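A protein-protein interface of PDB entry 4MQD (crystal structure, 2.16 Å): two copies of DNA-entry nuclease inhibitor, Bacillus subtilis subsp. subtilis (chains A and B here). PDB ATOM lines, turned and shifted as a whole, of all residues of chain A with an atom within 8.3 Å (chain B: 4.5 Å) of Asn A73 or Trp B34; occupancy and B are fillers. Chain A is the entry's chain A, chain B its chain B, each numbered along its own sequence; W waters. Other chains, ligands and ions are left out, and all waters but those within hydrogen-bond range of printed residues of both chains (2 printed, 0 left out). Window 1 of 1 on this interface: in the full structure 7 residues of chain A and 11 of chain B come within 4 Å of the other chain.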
ATOM      1  N   LEU A  63     -25.650 -16.226 -13.503  1.00  0.00           N
ATOM      2  CA  LEU A  63     -24.598 -17.180 -13.135  1.00  0.00           C
ATOM      3  C   LEU A  63     -23.523 -17.180 -14.209  1.00  0.00           C
ATOM      4  O   LEU A  63     -23.701 -17.781 -15.272  1.00  0.00           O
ATOM      5  CB  LEU A  63     -25.164 -18.596 -12.977  1.00  0.00           C
ATOM      6  CG  LEU A  63     -25.664 -18.976 -11.585  1.00  0.00           C
ATOM      7  CD1 LEU A  63     -26.732 -18.002 -11.112  1.00  0.00           C
ATOM      8  CD2 LEU A  63     -26.188 -20.406 -11.586  1.00  0.00           C
ATOM      9  N   ARG A  65     -19.841 -18.208 -15.677  1.00  0.00           N
ATOM     10  CA  ARG A  65     -18.877 -19.302 -15.572  1.00  0.00           C
ATOM     11  C   ARG A  65     -17.796 -19.194 -16.639  1.00  0.00           C
ATOM     12  O   ARG A  65     -18.039 -18.670 -17.728  1.00  0.00           O
ATOM     13  CB  ARG A  65     -19.581 -20.647 -15.734  1.00  0.00           C
ATOM     14  CG  ARG A  65     -20.613 -20.955 -14.666  1.00  0.00           C
ATOM     15  CD  ARG A  65     -21.327 -22.255 -14.975  1.00  0.00           C
ATOM     16  NE  ARG A  65     -22.386 -22.530 -14.013  1.00  0.00           N
ATOM     17  CZ  ARG A  65     -23.209 -23.574 -14.070  1.00  0.00           C
ATOM     18  NH1 ARG A  65     -23.111 -24.464 -15.052  1.00  0.00           N
ATOM     19  NH2 ARG A  65     -24.140 -23.726 -13.135  1.00  0.00           N
ATOM     20  N   GLU A  70     -20.052 -28.457 -16.430  1.00  0.00           N
ATOM     21  CA  GLU A  70     -21.324 -28.839 -15.823  1.00  0.00           C
ATOM     22  C   GLU A  70     -22.436 -28.675 -16.845  1.00  0.00           C
ATOM     23  O   GLU A  70     -22.654 -27.577 -17.358  1.00  0.00           O
ATOM     24  CB  GLU A  70     -21.641 -27.983 -14.590  1.00  0.00           C
ATOM     25  CG  GLU A  70     -20.880 -28.375 -13.331  1.00  0.00           C
ATOM     26  CD  GLU A  70     -21.470 -27.763 -12.067  1.00  0.00           C
ATOM     27  OE1 GLU A  70     -22.258 -26.797 -12.168  1.00  0.00           O
ATOM     28  OE2 GLU A  70     -21.140 -28.253 -10.964  1.00  0.00           O
ATOM     29  N   THR A  71     -23.135 -29.768 -17.143  1.00  0.00           N
ATOM     30  CA  THR A  71     -24.249 -29.722 -18.082  1.00  0.00           C
ATOM     31  C   THR A  71     -25.399 -28.917 -17.488  1.00  0.00           C
ATOM     32  O   THR A  71     -25.548 -28.834 -16.264  1.00  0.00           O
ATOM     33  CB  THR A  71     -24.758 -31.131 -18.450  1.00  0.00           C
ATOM     34  OG1 THR A  71     -25.166 -31.826 -17.265  1.00  0.00           O
ATOM     35  CG2 THR A  71     -23.669 -31.929 -19.156  1.00  0.00           C
ATOM     36  N   VAL A  72     -26.192 -28.311 -18.365  1.00  0.00           N
ATOM     37  CA  VAL A  72     -27.376 -27.564 -17.963  1.00  0.00           C
ATOM     38  C   VAL A  72     -28.592 -28.394 -18.358  1.00  0.00           C
ATOM     39  O   VAL A  72     -28.954 -28.465 -19.532  1.00  0.00           O
ATOM     40  CB  VAL A  72     -27.409 -26.176 -18.631  1.00  0.00           C
ATOM     41  CG1 VAL A  72     -28.630 -25.385 -18.176  1.00  0.00           C
ATOM     42  CG2 VAL A  72     -26.124 -25.420 -18.319  1.00  0.00           C
ATOM     43  N   ASN A  73     -29.208 -29.029 -17.365  1.00  0.00           N
ATOM     44  CA  ASN A  73     -30.266 -30.006 -17.606  1.00  0.00           C
ATOM     45  C   ASN A  73     -31.650 -29.390 -17.803  1.00  0.00           C
ATOM     46  O   ASN A  73     -32.563 -30.066 -18.274  1.00  0.00           O
ATOM     47  CB  ASN A  73     -30.304 -31.027 -16.466  1.00  0.00           C
ATOM     48  CG  ASN A  73     -29.078 -31.920 -16.445  1.00  0.00           C
ATOM     49  OD1 ASN A  73     -28.951 -32.834 -17.257  1.00  0.00           O
ATOM     50  ND2 ASN A  73     -28.166 -31.662 -15.514  1.00  0.00           N
ATOM     51  N   SER A  74     -31.804 -28.116 -17.445  1.00  0.00           N
ATOM     52  CA  SER A  74     -33.089 -27.430 -17.574  1.00  0.00           C
ATOM     53  C   SER A  74     -32.922 -26.028 -18.159  1.00  0.00           C
ATOM     54  O   SER A  74     -32.251 -25.182 -17.568  1.00  0.00           O
ATOM     55  CB  SER A  74     -33.777 -27.344 -16.211  1.00  0.00           C
ATOM     56  OG  SER A  74     -33.865 -28.621 -15.602  1.00  0.00           O
ATOM     57  N   TYR A  75     -33.532 -25.795 -19.320  1.00  0.00           N
ATOM     58  CA  TYR A  75     -33.543 -24.470 -19.948  1.00  0.00           C
ATOM     59  C   TYR A  75     -34.595 -24.376 -21.051  1.00  0.00           C
ATOM     60  O   TYR A  75     -35.046 -25.393 -21.578  1.00  0.00           O
ATOM     61  CB  TYR A  75     -32.165 -24.125 -20.523  1.00  0.00           C
ATOM     62  CG  TYR A  75     -31.665 -25.082 -21.584  1.00  0.00           C
ATOM     63  CD1 TYR A  75     -30.960 -26.233 -21.236  1.00  0.00           C
ATOM     64  CD2 TYR A  75     -31.878 -24.828 -22.938  1.00  0.00           C
ATOM     65  CE1 TYR A  75     -30.491 -27.106 -22.202  1.00  0.00           C
ATOM     66  CE2 TYR A  75     -31.414 -25.696 -23.911  1.00  0.00           C
ATOM     67  CZ  TYR A  75     -30.720 -26.833 -23.539  1.00  0.00           C
ATOM     68  OH  TYR A  75     -30.256 -27.698 -24.499  1.00  0.00           O
ATOM     69  N   GLU A  76     -34.978 -23.147 -21.389  1.00  0.00           N
ATOM     70  CA  GLU A  76     -35.936 -22.892 -22.464  1.00  0.00           C
ATOM     71  C   GLU A  76     -35.309 -22.199 -23.676  1.00  0.00           C
ATOM     72  O   GLU A  76     -35.967 -22.033 -24.702  1.00  0.00           O
ATOM     73  CB  GLU A  76     -37.107 -22.068 -21.931  1.00  0.00           C
ATOM     74  CG  GLU A  76     -37.993 -22.837 -20.965  1.00  0.00           C
ATOM     75  CD  GLU A  76     -39.360 -22.210 -20.780  1.00  0.00           C
ATOM     76  OE1 GLU A  76     -39.498 -20.982 -20.972  1.00  0.00           O
ATOM     77  OE2 GLU A  76     -40.302 -22.951 -20.431  1.00  0.00           O
ATOM     78  N   TRP A 114     -27.784 -19.752 -21.273  1.00  0.00           N
ATOM     79  CA  TRP A 114     -28.960 -20.590 -21.062  1.00  0.00           C
ATOM     80  C   TRP A 114     -30.011 -19.802 -20.296  1.00  0.00           C
ATOM     81  O   TRP A 114     -29.706 -19.210 -19.256  1.00  0.00           O
ATOM     82  CB  TRP A 114     -28.612 -21.843 -20.255  1.00  0.00           C
ATOM     83  CG  TRP A 114     -27.783 -22.862 -20.967  1.00  0.00           C
ATOM     84  CD1 TRP A 114     -28.235 -23.918 -21.706  1.00  0.00           C
ATOM     85  CD2 TRP A 114     -26.357 -22.951 -20.971  1.00  0.00           C
ATOM     86  NE1 TRP A 114     -27.175 -24.651 -22.184  1.00  0.00           N
ATOM     87  CE2 TRP A 114     -26.010 -24.080 -21.745  1.00  0.00           C
ATOM     88  CE3 TRP A 114     -25.338 -22.183 -20.400  1.00  0.00           C
ATOM     89  CZ2 TRP A 114     -24.684 -24.458 -21.965  1.00  0.00           C
ATOM     90  CZ3 TRP A 114     -24.021 -22.559 -20.616  1.00  0.00           C
ATOM     91  CH2 TRP A 114     -23.706 -23.685 -21.394  1.00  0.00           C
ATOM     92  N   VAL A 116     -33.004 -20.076 -17.922  1.00  0.00           N
ATOM     93  CA  VAL A 116     -33.616 -20.994 -16.961  1.00  0.00           C
ATOM     94  C   VAL A 116     -34.699 -20.249 -16.175  1.00  0.00           C
ATOM     95  O   VAL A 116     -34.392 -19.555 -15.202  1.00  0.00           O
ATOM     96  CB  VAL A 116     -32.565 -21.564 -15.982  1.00  0.00           C
ATOM     97  CG1 VAL A 116     -33.185 -22.634 -15.089  1.00  0.00           C
ATOM     98  CG2 VAL A 116     -31.372 -22.121 -16.746  1.00  0.00           C
ATOM     99  N   MET A 120     -37.997 -23.593 -13.331  1.00  0.00           N
ATOM    100  CA  MET A 120     -36.957 -24.618 -13.507  1.00  0.00           C
ATOM    101  C   MET A 120     -35.718 -24.380 -12.681  1.00  0.00           C
ATOM    102  O   MET A 120     -34.875 -25.268 -12.568  1.00  0.00           O
ATOM    103  CB  MET A 120     -36.486 -24.625 -14.958  1.00  0.00           C
ATOM    104  CG  MET A 120     -37.505 -25.241 -15.897  1.00  0.00           C
ATOM    105  SD  MET A 120     -36.813 -25.043 -17.728  1.00  0.00           S
ATOM    106  CE  MET A 120     -38.258 -26.000 -18.665  1.00  0.00           C
ATOM    107  N   SER A 121     -35.579 -23.185 -12.112  1.00  0.00           N
ATOM    108  CA  SER A 121     -34.368 -22.819 -11.377  1.00  0.00           C
ATOM    109  C   SER A 121     -34.476 -23.178  -9.902  1.00  0.00           C
ATOM    110  O   SER A 121     -35.528 -22.988  -9.286  1.00  0.00           O
ATOM    111  CB  SER A 121     -34.091 -21.320 -11.508  1.00  0.00           C
ATOM    112  OG  SER A 121     -32.903 -20.965 -10.822  1.00  0.00           O
ATOM    113  N   ASP A 122     -33.377 -23.671  -9.335  1.00  0.00           N
ATOM    114  CA  ASP A 122     -33.308 -23.946  -7.898  1.00  0.00           C
ATOM    115  C   ASP A 122     -33.096 -22.665  -7.078  1.00  0.00           C
ATOM    116  O   ASP A 122     -33.107 -22.704  -5.846  1.00  0.00           O
ATOM    117  CB  ASP A 122     -32.229 -24.993  -7.586  1.00  0.00           C
ATOM    118  CG  ASP A 122     -30.812 -24.512  -7.886  1.00  0.00           C
ATOM    119  OD1 ASP A 122     -30.635 -23.408  -8.444  1.00  0.00           O
ATOM    120  OD2 ASP A 122     -29.865 -25.257  -7.559  1.00  0.00           O
ATOM    121  N   ILE A 129     -27.658 -18.471 -17.129  1.00  0.00           N
ATOM    122  CA  ILE A 129     -26.336 -19.067 -16.978  1.00  0.00           C
ATOM    123  C   ILE A 129     -25.494 -18.674 -18.181  1.00  0.00           C
ATOM    124  O   ILE A 129     -25.893 -18.902 -19.324  1.00  0.00           O
ATOM    125  CB  ILE A 129     -26.402 -20.605 -16.866  1.00  0.00           C
ATOM    126  CG1 ILE A 129     -27.290 -21.015 -15.683  1.00  0.00           C
ATOM    127  CG2 ILE A 129     -25.000 -21.191 -16.713  1.00  0.00           C
ATOM    128  CD1 ILE A 129     -27.541 -22.505 -15.580  1.00  0.00           C
ATOM    129  N   TYR B  17     -31.768 -33.137 -23.160  1.00  0.00           N
ATOM    130  CA  TYR B  17     -31.327 -32.392 -21.977  1.00  0.00           C
ATOM    131  C   TYR B  17     -30.471 -33.230 -21.017  1.00  0.00           C
ATOM    132  O   TYR B  17     -30.552 -33.074 -19.797  1.00  0.00           O
ATOM    133  CB  TYR B  17     -32.538 -31.783 -21.260  1.00  0.00           C
ATOM    134  CG  TYR B  17     -33.295 -30.816 -22.138  1.00  0.00           C
ATOM    135  CD1 TYR B  17     -34.288 -31.264 -23.007  1.00  0.00           C
ATOM    136  CD2 TYR B  17     -32.999 -29.457 -22.125  1.00  0.00           C
ATOM    137  CE1 TYR B  17     -34.974 -30.383 -23.825  1.00  0.00           C
ATOM    138  CE2 TYR B  17     -33.679 -28.567 -22.941  1.00  0.00           C
ATOM    139  CZ  TYR B  17     -34.664 -29.035 -23.787  1.00  0.00           C
ATOM    140  OH  TYR B  17     -35.340 -28.156 -24.601  1.00  0.00           O
ATOM    141  N   HIS B  18     -29.647 -34.109 -21.591  1.00  0.00           N
ATOM    142  CA  HIS B  18     -28.688 -34.925 -20.844  1.00  0.00           C
ATOM    143  C   HIS B  18     -29.293 -35.613 -19.619  1.00  0.00           C
ATOM    144  O   HIS B  18     -28.682 -35.640 -18.546  1.00  0.00           O
ATOM    145  CB  HIS B  18     -27.484 -34.072 -20.432  1.00  0.00           C
ATOM    146  CG  HIS B  18     -26.642 -33.628 -21.584  1.00  0.00           C
ATOM    147  ND1 HIS B  18     -26.685 -32.347 -22.090  1.00  0.00           N
ATOM    148  CD2 HIS B  18     -25.735 -34.298 -22.332  1.00  0.00           C
ATOM    149  CE1 HIS B  18     -25.839 -32.246 -23.100  1.00  0.00           C
ATOM    150  NE2 HIS B  18     -25.250 -33.416 -23.268  1.00  0.00           N
ATOM    151  N   GLN B  19     -30.486 -36.179 -19.785  1.00  0.00           N
ATOM    152  CA  GLN B  19     -31.170 -36.826 -18.674  1.00  0.00           C
ATOM    153  C   GLN B  19     -32.249 -37.819 -19.096  1.00  0.00           C
ATOM    154  O   GLN B  19     -32.777 -37.757 -20.208  1.00  0.00           O
ATOM    155  CB  GLN B  19     -31.805 -35.769 -17.767  1.00  0.00           C
ATOM    156  CG  GLN B  19     -32.886 -34.940 -18.445  1.00  0.00           C
ATOM    157  CD  GLN B  19     -33.534 -33.954 -17.501  1.00  0.00           C
ATOM    158  OE1 GLN B  19     -33.248 -32.758 -17.542  1.00  0.00           O
ATOM    159  NE2 GLN B  19     -34.406 -34.452 -16.637  1.00  0.00           N
ATOM    160  N   MET B  32     -36.704 -31.370 -10.705  1.00  0.00           N
ATOM    161  CA  MET B  32     -35.468 -31.772 -10.031  1.00  0.00           C
ATOM    162  C   MET B  32     -34.608 -30.583  -9.719  1.00  0.00           C
ATOM    163  O   MET B  32     -34.599 -29.591 -10.454  1.00  0.00           O
ATOM    164  CB  MET B  32     -34.667 -32.744 -10.893  1.00  0.00           C
ATOM    165  CG  MET B  32     -35.385 -34.079 -11.068  1.00  0.00           C
ATOM    166  SD  MET B  32     -35.555 -35.022  -9.347  1.00  0.00           S
ATOM    167  CE  MET B  32     -36.593 -36.575  -9.973  1.00  0.00           C
ATOM    168  N   ASP B  33     -33.873 -30.684  -8.615  1.00  0.00           N
ATOM    169  CA  ASP B  33     -32.930 -29.657  -8.202  1.00  0.00           C
ATOM    170  C   ASP B  33     -31.535 -30.064  -8.677  1.00  0.00           C
ATOM    171  O   ASP B  33     -30.837 -30.828  -8.008  1.00  0.00           O
ATOM    172  CB  ASP B  33     -32.971 -29.490  -6.677  1.00  0.00           C
ATOM    173  CG  ASP B  33     -32.235 -28.250  -6.196  1.00  0.00           C
ATOM    174  OD1 ASP B  33     -31.332 -27.763  -6.910  1.00  0.00           O
ATOM    175  OD2 ASP B  33     -32.558 -27.764  -5.092  1.00  0.00           O
ATOM    176  N   TRP B  34     -31.141 -29.555  -9.842  1.00  0.00           N
ATOM    177  CA  TRP B  34     -29.840 -29.880 -10.422  1.00  0.00           C
ATOM    178  C   TRP B  34     -28.747 -28.995  -9.835  1.00  0.00           C
ATOM    179  O   TRP B  34     -28.298 -28.036 -10.466  1.00  0.00           O
ATOM    180  CB  TRP B  34     -29.871 -29.742 -11.947  1.00  0.00           C
ATOM    181  CG  TRP B  34     -30.705 -30.781 -12.618  1.00  0.00           C
ATOM    182  CD1 TRP B  34     -31.927 -30.601 -13.198  1.00  0.00           C
ATOM    183  CD2 TRP B  34     -30.385 -32.167 -12.777  1.00  0.00           C
ATOM    184  NE1 TRP B  34     -32.385 -31.789 -13.712  1.00  0.00           N
ATOM    185  CE2 TRP B  34     -31.459 -32.767 -13.468  1.00  0.00           C
ATOM    186  CE3 TRP B  34     -29.291 -32.960 -12.406  1.00  0.00           C
ATOM    187  CZ2 TRP B  34     -31.474 -34.126 -13.796  1.00  0.00           C
ATOM    188  CZ3 TRP B  34     -29.307 -34.313 -12.732  1.00  0.00           C
ATOM    189  CH2 TRP B  34     -30.391 -34.881 -13.421  1.00  0.00           C
ATOM    190  N   THR B  35     -28.327 -29.329  -8.618  1.00  0.00           N
ATOM    191  CA  THR B  35     -27.231 -28.634  -7.956  1.00  0.00           C
ATOM    192  C   THR B  35     -25.901 -29.101  -8.532  1.00  0.00           C
ATOM    193  O   THR B  35     -25.839 -30.112  -9.241  1.00  0.00           O
ATOM    194  CB  THR B  35     -27.226 -28.909  -6.442  1.00  0.00           C
ATOM    195  OG1 THR B  35     -27.106 -30.319  -6.209  1.00  0.00           O
ATOM    196  CG2 THR B  35     -28.503 -28.401  -5.800  1.00  0.00           C
ATOM    197  N   ASP B  36     -24.839 -28.364  -8.219  1.00  0.00           N
ATOM    198  CA  ASP B  36     -23.485 -28.753  -8.615  1.00  0.00           C
ATOM    199  C   ASP B  36     -23.191 -30.183  -8.170  1.00  0.00           C
ATOM    200  O   ASP B  36     -22.668 -30.984  -8.943  1.00  0.00           O
ATOM    201  CB  ASP B  36     -22.447 -27.801  -8.009  1.00  0.00           C
ATOM    202  CG  ASP B  36     -22.517 -26.401  -8.596  1.00  0.00           C
ATOM    203  OD1 ASP B  36     -23.399 -26.143  -9.443  1.00  0.00           O
ATOM    204  OD2 ASP B  36     -21.686 -25.555  -8.205  1.00  0.00           O
ATOM    205  N   ALA B  38     -25.408 -32.652  -7.320  1.00  0.00           N
ATOM    206  CA  ALA B  38     -26.260 -33.590  -8.062  1.00  0.00           C
ATOM    207  C   ALA B  38     -25.687 -33.910  -9.443  1.00  0.00           C
ATOM    208  O   ALA B  38     -25.669 -35.069  -9.865  1.00  0.00           O
ATOM    209  CB  ALA B  38     -27.669 -33.033  -8.195  1.00  0.00           C
ATOM    210  N   ILE B  39     -25.216 -32.875 -10.134  1.00  0.00           N
ATOM    211  CA  ILE B  39     -24.598 -33.032 -11.450  1.00  0.00           C
ATOM    212  C   ILE B  39     -23.299 -33.837 -11.337  1.00  0.00           C
ATOM    213  O   ILE B  39     -23.045 -34.727 -12.151  1.00  0.00           O
ATOM    214  CB  ILE B  39     -24.321 -31.659 -12.110  1.00  0.00           C
ATOM    215  CG1 ILE B  39     -25.639 -30.921 -12.386  1.00  0.00           C
ATOM    216  CG2 ILE B  39     -23.539 -31.823 -13.409  1.00  0.00           C
ATOM    217  CD1 ILE B  39     -25.490 -29.417 -12.493  1.00  0.00           C
ATOM    218  N   TYR B  43     -26.732 -37.843 -10.721  1.00  0.00           N
ATOM    219  CA  TYR B  43     -28.176 -38.045 -10.577  1.00  0.00           C
ATOM    220  C   TYR B  43     -28.822 -37.022  -9.645  1.00  0.00           C
ATOM    221  O   TYR B  43     -28.150 -36.411  -8.811  1.00  0.00           O
ATOM    222  CB  TYR B  43     -28.481 -39.461 -10.069  1.00  0.00           C
ATOM    223  CG  TYR B  43     -28.140 -39.684  -8.611  1.00  0.00           C
ATOM    224  CD1 TYR B  43     -26.847 -40.025  -8.223  1.00  0.00           C
ATOM    225  CD2 TYR B  43     -29.111 -39.558  -7.619  1.00  0.00           C
ATOM    226  CE1 TYR B  43     -26.529 -40.233  -6.890  1.00  0.00           C
ATOM    227  CE2 TYR B  43     -28.802 -39.763  -6.283  1.00  0.00           C
ATOM    228  CZ  TYR B  43     -27.510 -40.101  -5.925  1.00  0.00           C
ATOM    229  OH  TYR B  43     -27.195 -40.305  -4.602  1.00  0.00           O
ATOM    230  N   ALA B  44     -30.133 -36.853  -9.799  1.00  0.00           N
ATOM    231  CA  ALA B  44     -30.939 -36.033  -8.897  1.00  0.00           C
ATOM    232  C   ALA B  44     -32.162 -36.827  -8.468  1.00  0.00           C
ATOM    233  O   ALA B  44     -32.816 -37.457  -9.298  1.00  0.00           O
ATOM    234  CB  ALA B  44     -31.362 -34.745  -9.584  1.00  0.00           C
ATOM    235  N   SER B  51     -33.638 -38.843 -11.525  1.00  0.00           N
ATOM    236  CA  SER B  51     -33.187 -38.427 -12.851  1.00  0.00           C
ATOM    237  C   SER B  51     -31.693 -38.688 -12.972  1.00  0.00           C
ATOM    238  O   SER B  51     -30.904 -38.139 -12.206  1.00  0.00           O
ATOM    239  CB  SER B  51     -33.478 -36.944 -13.089  1.00  0.00           C
ATOM    240  OG  SER B  51     -34.871 -36.705 -13.186  1.00  0.00           O
ATOM    241  N   GLU B  53     -28.103 -38.456 -15.006  1.00  0.00           N
ATOM    242  CA  GLU B  53     -27.343 -37.748 -16.038  1.00  0.00           C
ATOM    243  C   GLU B  53     -27.018 -38.707 -17.183  1.00  0.00           C
ATOM    244  O   GLU B  53     -26.571 -39.833 -16.949  1.00  0.00           O
ATOM    245  CB  GLU B  53     -26.036 -37.183 -15.472  1.00  0.00           C
ATOM    246  CG  GLU B  53     -26.206 -36.018 -14.507  1.00  0.00           C
ATOM    247  CD  GLU B  53     -26.546 -34.703 -15.190  1.00  0.00           C
ATOM    248  OE1 GLU B  53     -26.585 -34.651 -16.439  1.00  0.00           O
ATOM    249  OE2 GLU B  53     -26.768 -33.709 -14.465  1.00  0.00           O
ATOM    250  N   ILE B  95     -37.075 -35.989 -21.587  1.00  0.00           N
ATOM    251  CA  ILE B  95     -37.895 -34.819 -21.902  1.00  0.00           C
ATOM    252  C   ILE B  95     -38.471 -34.913 -23.323  1.00  0.00           C
ATOM    253  O   ILE B  95     -37.735 -34.864 -24.309  1.00  0.00           O
ATOM    254  CB  ILE B  95     -37.112 -33.500 -21.706  1.00  0.00           C
ATOM    255  CG1 ILE B  95     -36.704 -33.353 -20.232  1.00  0.00           C
ATOM    256  CG2 ILE B  95     -37.960 -32.306 -22.135  1.00  0.00           C
ATOM    257  CD1 ILE B  95     -35.773 -32.201 -19.932  1.00  0.00           C
HETATM  258  O   HOH W   1     -28.567 -30.611 -21.193  1.00  0.00           O
HETATM  259  O   HOH W   2     -34.722 -28.125 -13.044  1.00  0.00           O
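The side-chain hydroxyl (OG1) of Thr A71 is in hydrogen-bond range of the side-chain carboxylate (OE1) of Glu B53 (3.3 Å). The side-chain amide oxygen (OD1) of Asn A73 sits close to the backbone carbonyl oxygen (O) of Tyr B17 (3.0 Å). The backbone carbonyl oxygen of His B18 lies close to the side-chain amide oxygen of Asn A73 (3.1 Å). OE1 of Gln B19 sits close to O of Asn A73, at 2.9 Å. ND2 of Asn A73 is in hydrogen-bond range of OE2 of Glu B53 (2.7 Å). The side-chain carboxylate of Asp B36 sits close to the side-chain carboxylate of Glu A70, at 3.0 Å. OD2 of Asp A122 lies close to OD1 of Asp B33 (3.0 Å).
OE1 of Glu A70 is in salt-bridge range of NH2 of Arg A65 (3.7 Å). OG1 of Thr A71 lies within hydrogen-bond range of ND2 of Asn A73, 3.5 Å away. SD of Met A120 lies within hydrogen-bond range of N of Tyr A75 (3.7 Å). N of Ala B38 sits at hydrogen-bond distance from OG1 of Thr B35, 3.1 Å away.
Among the printed residues, merely in contact across the chains: Thr A71 with Ile B39 (3.8 Å), Asn A73 with Trp B34 (3.5 Å), Ser A74 with Trp B34 (3.7 Å), Tyr A75 with Tyr B17 (3.4 Å) and Asp A122 with Thr B35 (3.9 Å).
Leu A63 touches none of the printed residues of chain B. Printed residues of chain B within 4 Å of Thr A71: Ile B39 and Glu B53. Of chain B, only Tyr B17 (3.0 Å), His B18 (3.1 Å), Gln B19 (2.9 Å), Trp B34 (3.5 Å) and Glu B53 (2.7 Å) come within 4 Å of Asn A73. Of the printed residues of chain A, His B18 touches Asn A73 (3.1 Å). Printed residues of chain A within 4 Å of Asp B33: Asp A122. Of the printed residues of chain A, Trp B34 touches Asn A73 (3.5 Å) and Ser A74 (3.7 Å). Thr B35 touches just one residue of chain A: Asp A122 (3.9 Å). Printed residues of chain A within 4 Å of Glu B53: Thr A71 (3.3 Å) and Asn A73 (2.7 Å). The nearest residue of chain B that does not touch Asn A73 is Ile B39 (4.1 Å). The nearest residue of chain A that does not touch Trp B34 is Asp A122 (4.3 Å).
Of the 15 printed residues of chain B, 9 touch a printed residue of chain A. Of the 15 printed residues of chain A, 6 touch a printed residue of chain B. Printed residues of chain A that touch a printed residue of chain B: Glu A70, Thr A71, Asn A73, Ser A74, Tyr A75 and Asp A122. Hydrophobic or aromatic side chains of chain A within 4 Å of the printed part of chain B: Tyr A75. Along chain A the printed residues that touch a printed residue of chain B span positions 70 to 122. Among the printed residues, 12 pairs touch across the chains. Among the printed residues, no Asp or Glu carboxylate lies within 4 Å of a Lys or Arg side-chain nitrogen of the other chain.
No position is printed for both chains.
Water W1 lies within hydrogen-bond range of ND1 of His B18 (2.7 Å), O of Val A72 (2.7 Å) and O of Tyr B17 (3.5 Å). Water W2 lies within hydrogen-bond range of the side-chain hydroxyl of Ser A74, the backbone carbonyl oxygen of Met A120 and the backbone carbonyl oxygen of Met B32.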
